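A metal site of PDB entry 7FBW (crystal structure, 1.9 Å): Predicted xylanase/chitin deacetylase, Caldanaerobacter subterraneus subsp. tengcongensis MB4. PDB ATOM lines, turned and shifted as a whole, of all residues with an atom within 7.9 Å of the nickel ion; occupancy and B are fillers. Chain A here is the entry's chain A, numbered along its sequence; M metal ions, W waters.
A ring nitrogen (ND1) of His 175 is in hydrogen-bond range of the backbone carbonyl oxygen (O) of Arg 213. NE2 of His 175 lies close to OD2 of Asp 124 (3.5 Å). N of Asp 125 is in hydrogen-bond range of O of Phe 149, at 2.9 Å. The backbone NH of His 179 lies within hydrogen-bond range of the side-chain hydroxyl of Ser 176, at 2.8 Å.
Of the 19 residues printed, 3 come within 4 Å of the nickel ion. The nearest printed residue that does not touch the nickel ion is Asp 124 (4.1 Å).
The nickel ion is bound by water W2 (1.9 Å), the side-chain carboxylate of Asp 125 (1.9 Å), water W3 (2.1 Å), a ring nitrogen (NE2) of His 179 (2.1 Å), a ring nitrogen (NE2) of His 175 (2.1 Å) and water W1 (2.2 Å). The nickel ion has six donor atoms within binding distance.
Water W3 bridges the side-chain carboxylate of Asp 124 (2.6 Å) and a ring nitrogen (NE2) of His 269 (3.1 Å).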
ATOM      1  N   PHE A 123      33.974 -16.936 -25.129  1.00  0.00           N
ATOM      2  CA  PHE A 123      32.563 -16.493 -25.012  1.00  0.00           C
ATOM      3  C   PHE A 123      31.613 -17.515 -25.628  1.00  0.00           C
ATOM      4  O   PHE A 123      31.702 -17.682 -26.850  1.00  0.00           O
ATOM      5  CB  PHE A 123      32.458 -15.169 -25.774  1.00  0.00           C
ATOM      6  CG  PHE A 123      33.427 -14.165 -25.221  1.00  0.00           C
ATOM      7  CD1 PHE A 123      33.267 -13.735 -23.923  1.00  0.00           C
ATOM      8  CD2 PHE A 123      34.510 -13.721 -25.962  1.00  0.00           C
ATOM      9  CE1 PHE A 123      34.137 -12.782 -23.395  1.00  0.00           C
ATOM     10  CE2 PHE A 123      35.405 -12.790 -25.415  1.00  0.00           C
ATOM     11  CZ  PHE A 123      35.215 -12.353 -24.123  1.00  0.00           C
ATOM     12  N   ASP A 124      30.688 -18.007 -24.824  1.00  0.00           N
ATOM     13  CA  ASP A 124      29.649 -18.999 -25.199  1.00  0.00           C
ATOM     14  C   ASP A 124      28.339 -18.294 -25.550  1.00  0.00           C
ATOM     15  O   ASP A 124      28.097 -17.162 -25.023  1.00  0.00           O
ATOM     16  CB  ASP A 124      29.329 -19.907 -24.025  1.00  0.00           C
ATOM     17  CG  ASP A 124      30.291 -21.081 -23.889  1.00  0.00           C
ATOM     18  OD1 ASP A 124      31.335 -21.008 -24.559  1.00  0.00           O
ATOM     19  OD2 ASP A 124      30.012 -21.960 -23.021  1.00  0.00           O
ATOM     20  N   ASP A 125      27.557 -18.940 -26.419  1.00  0.00           N
ATOM     21  CA  ASP A 125      26.084 -18.872 -26.522  1.00  0.00           C
ATOM     22  C   ASP A 125      25.648 -17.844 -27.561  1.00  0.00           C
ATOM     23  O   ASP A 125      24.455 -17.730 -27.744  1.00  0.00           O
ATOM     24  CB  ASP A 125      25.409 -18.543 -25.201  1.00  0.00           C
ATOM     25  CG  ASP A 125      25.370 -19.621 -24.157  1.00  0.00           C
ATOM     26  OD1 ASP A 125      24.824 -19.290 -23.119  1.00  0.00           O
ATOM     27  OD2 ASP A 125      25.892 -20.801 -24.356  1.00  0.00           O
ATOM     28  N   GLY A 126      26.576 -17.214 -28.278  1.00  0.00           N
ATOM     29  CA  GLY A 126      26.250 -16.225 -29.316  1.00  0.00           C
ATOM     30  C   GLY A 126      26.056 -16.876 -30.678  1.00  0.00           C
ATOM     31  O   GLY A 126      25.911 -18.114 -30.789  1.00  0.00           O
ATOM     32  N   PHE A 149      32.262 -19.636 -28.865  1.00  0.00           N
ATOM     33  CA  PHE A 149      31.557 -20.924 -29.024  1.00  0.00           C
ATOM     34  C   PHE A 149      30.076 -20.611 -29.258  1.00  0.00           C
ATOM     35  O   PHE A 149      29.282 -20.378 -28.253  1.00  0.00           O
ATOM     36  CB  PHE A 149      31.797 -21.796 -27.802  1.00  0.00           C
ATOM     37  CG  PHE A 149      33.212 -22.276 -27.685  1.00  0.00           C
ATOM     38  CD1 PHE A 149      34.109 -21.639 -26.873  1.00  0.00           C
ATOM     39  CD2 PHE A 149      33.620 -23.440 -28.356  1.00  0.00           C
ATOM     40  CE1 PHE A 149      35.409 -22.095 -26.746  1.00  0.00           C
ATOM     41  CE2 PHE A 149      34.922 -23.880 -28.259  1.00  0.00           C
ATOM     42  CZ  PHE A 149      35.833 -23.214 -27.454  1.00  0.00           C
ATOM     43  N   ILE A 151      26.118 -20.995 -30.672  1.00  0.00           N
ATOM     44  CA  ILE A 151      24.961 -21.895 -30.792  1.00  0.00           C
ATOM     45  C   ILE A 151      24.475 -21.836 -32.226  1.00  0.00           C
ATOM     46  O   ILE A 151      24.253 -20.738 -32.727  1.00  0.00           O
ATOM     47  CB  ILE A 151      23.873 -21.493 -29.796  1.00  0.00           C
ATOM     48  CG1 ILE A 151      24.340 -21.694 -28.363  1.00  0.00           C
ATOM     49  CG2 ILE A 151      22.556 -22.229 -30.051  1.00  0.00           C
ATOM     50  CD1 ILE A 151      23.460 -20.976 -27.349  1.00  0.00           C
ATOM     51  N   HIS A 175      29.027 -24.711 -30.164  1.00  0.00           N
ATOM     52  CA  HIS A 175      28.380 -24.919 -28.845  1.00  0.00           C
ATOM     53  C   HIS A 175      27.077 -25.714 -29.033  1.00  0.00           C
ATOM     54  O   HIS A 175      26.193 -25.619 -28.187  1.00  0.00           O
ATOM     55  CB  HIS A 175      28.153 -23.545 -28.165  1.00  0.00           C
ATOM     56  CG  HIS A 175      27.907 -23.612 -26.693  1.00  0.00           C
ATOM     57  ND1 HIS A 175      28.502 -24.571 -25.857  1.00  0.00           N
ATOM     58  CD2 HIS A 175      27.126 -22.840 -25.895  1.00  0.00           C
ATOM     59  CE1 HIS A 175      28.097 -24.337 -24.597  1.00  0.00           C
ATOM     60  NE2 HIS A 175      27.242 -23.292 -24.628  1.00  0.00           N
ATOM     61  N   SER A 176      26.988 -26.516 -30.092  1.00  0.00           N
ATOM     62  CA  SER A 176      25.813 -27.325 -30.534  1.00  0.00           C
ATOM     63  C   SER A 176      24.814 -26.445 -31.302  1.00  0.00           C
ATOM     64  O   SER A 176      24.988 -25.211 -31.397  1.00  0.00           O
ATOM     65  CB  SER A 176      25.116 -28.064 -29.406  1.00  0.00           C
ATOM     66  OG  SER A 176      24.205 -27.212 -28.734  1.00  0.00           O
ATOM     67  N   HIS A 179      21.608 -26.240 -28.228  1.00  0.00           N
ATOM     68  CA  HIS A 179      22.012 -25.875 -26.839  1.00  0.00           C
ATOM     69  C   HIS A 179      21.254 -26.718 -25.815  1.00  0.00           C
ATOM     70  O   HIS A 179      21.036 -26.238 -24.728  1.00  0.00           O
ATOM     71  CB  HIS A 179      21.846 -24.367 -26.607  1.00  0.00           C
ATOM     72  CG  HIS A 179      22.615 -23.783 -25.444  1.00  0.00           C
ATOM     73  ND1 HIS A 179      22.027 -22.889 -24.543  1.00  0.00           N
ATOM     74  CD2 HIS A 179      23.926 -23.830 -25.110  1.00  0.00           C
ATOM     75  CE1 HIS A 179      22.947 -22.473 -23.678  1.00  0.00           C
ATOM     76  NE2 HIS A 179      24.125 -23.041 -24.003  1.00  0.00           N
ATOM     77  N   ARG A 213      32.605 -27.019 -27.622  1.00  0.00           N
ATOM     78  CA  ARG A 213      32.340 -26.958 -26.183  1.00  0.00           C
ATOM     79  C   ARG A 213      30.924 -27.441 -25.963  1.00  0.00           C
ATOM     80  O   ARG A 213      29.969 -26.827 -26.414  1.00  0.00           O
ATOM     81  CB  ARG A 213      32.469 -25.526 -25.633  1.00  0.00           C
ATOM     82  CG  ARG A 213      32.190 -25.482 -24.139  1.00  0.00           C
ATOM     83  CD  ARG A 213      32.555 -24.098 -23.623  1.00  0.00           C
ATOM     84  NE  ARG A 213      33.958 -23.837 -23.449  1.00  0.00           N
ATOM     85  CZ  ARG A 213      34.519 -22.607 -23.358  1.00  0.00           C
ATOM     86  NH1 ARG A 213      33.765 -21.552 -23.561  1.00  0.00           N
ATOM     87  NH2 ARG A 213      35.799 -22.452 -23.106  1.00  0.00           N
ATOM     88  N   PRO A 214      30.720 -28.559 -25.253  1.00  0.00           N
ATOM     89  CA  PRO A 214      29.348 -29.039 -25.059  1.00  0.00           C
ATOM     90  C   PRO A 214      28.566 -28.094 -24.167  1.00  0.00           C
ATOM     91  O   PRO A 214      29.099 -27.545 -23.183  1.00  0.00           O
ATOM     92  CB  PRO A 214      29.467 -30.375 -24.353  1.00  0.00           C
ATOM     93  CG  PRO A 214      30.918 -30.760 -24.628  1.00  0.00           C
ATOM     94  CD  PRO A 214      31.739 -29.459 -24.695  1.00  0.00           C
ATOM     95  N   PRO A 215      27.253 -27.959 -24.426  1.00  0.00           N
ATOM     96  CA  PRO A 215      26.371 -27.294 -23.478  1.00  0.00           C
ATOM     97  C   PRO A 215      26.487 -27.880 -22.063  1.00  0.00           C
ATOM     98  O   PRO A 215      26.433 -29.129 -21.868  1.00  0.00           O
ATOM     99  CB  PRO A 215      24.972 -27.609 -24.043  1.00  0.00           C
ATOM    100  CG  PRO A 215      25.229 -27.731 -25.559  1.00  0.00           C
ATOM    101  CD  PRO A 215      26.547 -28.454 -25.633  1.00  0.00           C
ATOM    102  N   PHE A 216      26.629 -26.974 -21.099  1.00  0.00           N
ATOM    103  CA  PHE A 216      26.794 -27.255 -19.653  1.00  0.00           C
ATOM    104  C   PHE A 216      28.113 -28.005 -19.416  1.00  0.00           C
ATOM    105  O   PHE A 216      28.337 -28.489 -18.335  1.00  0.00           O
ATOM    106  CB  PHE A 216      25.598 -28.027 -19.114  1.00  0.00           C
ATOM    107  CG  PHE A 216      24.281 -27.405 -19.520  1.00  0.00           C
ATOM    108  CD1 PHE A 216      23.952 -26.144 -19.072  1.00  0.00           C
ATOM    109  CD2 PHE A 216      23.414 -28.053 -20.397  1.00  0.00           C
ATOM    110  CE1 PHE A 216      22.766 -25.554 -19.474  1.00  0.00           C
ATOM    111  CE2 PHE A 216      22.233 -27.447 -20.811  1.00  0.00           C
ATOM    112  CZ  PHE A 216      21.911 -26.202 -20.330  1.00  0.00           C
ATOM    113  N   GLY A 217      28.943 -28.186 -20.455  1.00  0.00           N
ATOM    114  CA  GLY A 217      30.152 -29.021 -20.289  1.00  0.00           C
ATOM    115  C   GLY A 217      29.806 -30.496 -20.124  1.00  0.00           C
ATOM    116  O   GLY A 217      30.656 -31.254 -19.682  1.00  0.00           O
ATOM    117  N   TRP A 237      36.743 -25.746 -19.979  1.00  0.00           N
ATOM    118  CA  TRP A 237      37.284 -24.485 -19.437  1.00  0.00           C
ATOM    119  C   TRP A 237      37.914 -24.820 -18.092  1.00  0.00           C
ATOM    120  O   TRP A 237      37.769 -25.990 -17.630  1.00  0.00           O
ATOM    121  CB  TRP A 237      36.192 -23.425 -19.311  1.00  0.00           C
ATOM    122  CG  TRP A 237      35.107 -23.857 -18.375  1.00  0.00           C
ATOM    123  CD1 TRP A 237      35.131 -23.806 -17.014  1.00  0.00           C
ATOM    124  CD2 TRP A 237      33.903 -24.571 -18.733  1.00  0.00           C
ATOM    125  NE1 TRP A 237      34.007 -24.377 -16.494  1.00  0.00           N
ATOM    126  CE2 TRP A 237      33.226 -24.845 -17.539  1.00  0.00           C
ATOM    127  CE3 TRP A 237      33.327 -24.991 -19.938  1.00  0.00           C
ATOM    128  CZ2 TRP A 237      31.994 -25.526 -17.525  1.00  0.00           C
ATOM    129  CZ3 TRP A 237      32.107 -25.637 -19.925  1.00  0.00           C
ATOM    130  CH2 TRP A 237      31.445 -25.918 -18.717  1.00  0.00           C
ATOM    131  N   TRP A 244      27.354 -16.049 -15.950  1.00  0.00           N
ATOM    132  CA  TRP A 244      25.993 -16.379 -16.452  1.00  0.00           C
ATOM    133  C   TRP A 244      24.963 -15.812 -15.491  1.00  0.00           C
ATOM    134  O   TRP A 244      24.142 -15.059 -15.974  1.00  0.00           O
ATOM    135  CB  TRP A 244      25.724 -17.871 -16.695  1.00  0.00           C
ATOM    136  CG  TRP A 244      24.531 -18.025 -17.593  1.00  0.00           C
ATOM    137  CD1 TRP A 244      24.500 -17.836 -18.944  1.00  0.00           C
ATOM    138  CD2 TRP A 244      23.183 -18.315 -17.191  1.00  0.00           C
ATOM    139  NE1 TRP A 244      23.225 -18.045 -19.423  1.00  0.00           N
ATOM    140  CE2 TRP A 244      22.394 -18.339 -18.371  1.00  0.00           C
ATOM    141  CE3 TRP A 244      22.558 -18.596 -15.966  1.00  0.00           C
ATOM    142  CZ2 TRP A 244      21.027 -18.620 -18.359  1.00  0.00           C
ATOM    143  CZ3 TRP A 244      21.203 -18.870 -15.956  1.00  0.00           C
ATOM    144  CH2 TRP A 244      20.455 -18.879 -17.132  1.00  0.00           C
ATOM    145  N   LEU A 267      35.903 -19.229 -19.113  1.00  0.00           N
ATOM    146  CA  LEU A 267      34.514 -19.321 -19.584  1.00  0.00           C
ATOM    147  C   LEU A 267      33.804 -17.981 -19.291  1.00  0.00           C
ATOM    148  O   LEU A 267      33.542 -17.712 -18.103  1.00  0.00           O
ATOM    149  CB  LEU A 267      33.825 -20.475 -18.872  1.00  0.00           C
ATOM    150  CG  LEU A 267      32.314 -20.573 -19.126  1.00  0.00           C
ATOM    151  CD1 LEU A 267      32.008 -20.911 -20.585  1.00  0.00           C
ATOM    152  CD2 LEU A 267      31.641 -21.553 -18.164  1.00  0.00           C
ATOM    153  N   MET A 268      33.411 -17.276 -20.344  1.00  0.00           N
ATOM    154  CA  MET A 268      32.464 -16.133 -20.248  1.00  0.00           C
ATOM    155  C   MET A 268      31.361 -16.320 -21.293  1.00  0.00           C
ATOM    156  O   MET A 268      31.415 -17.298 -22.108  1.00  0.00           O
ATOM    157  CB  MET A 268      33.210 -14.820 -20.465  1.00  0.00           C
ATOM    158  CG  MET A 268      34.466 -14.776 -19.607  1.00  0.00           C
ATOM    159  SD  MET A 268      35.151 -13.119 -19.483  1.00  0.00           S
ATOM    160  CE  MET A 268      34.149 -12.625 -18.077  1.00  0.00           C
ATOM    161  N   HIS A 269      30.350 -15.476 -21.196  1.00  0.00           N
ATOM    162  CA  HIS A 269      29.111 -15.571 -21.995  1.00  0.00           C
ATOM    163  C   HIS A 269      28.982 -14.331 -22.820  1.00  0.00           C
ATOM    164  O   HIS A 269      29.304 -13.230 -22.324  1.00  0.00           O
ATOM    165  CB  HIS A 269      27.928 -15.842 -21.088  1.00  0.00           C
ATOM    166  CG  HIS A 269      27.953 -17.248 -20.608  1.00  0.00           C
ATOM    167  ND1 HIS A 269      28.676 -17.648 -19.512  1.00  0.00           N
ATOM    168  CD2 HIS A 269      27.302 -18.339 -21.059  1.00  0.00           C
ATOM    169  CE1 HIS A 269      28.454 -18.931 -19.287  1.00  0.00           C
ATOM    170  NE2 HIS A 269      27.664 -19.395 -20.266  1.00  0.00           N
HETATM  171 NI    NI M   1      25.947 -22.355 -23.193  1.00  0.00          NI
HETATM  172  O   HOH W   1      24.732 -21.451 -21.597  1.00  0.00           O
HETATM  173  O   HOH W   2      25.936 -23.958 -22.101  1.00  0.00           O
HETATM  174  O   HOH W   3      27.617 -21.849 -22.096  1.00  0.00           O
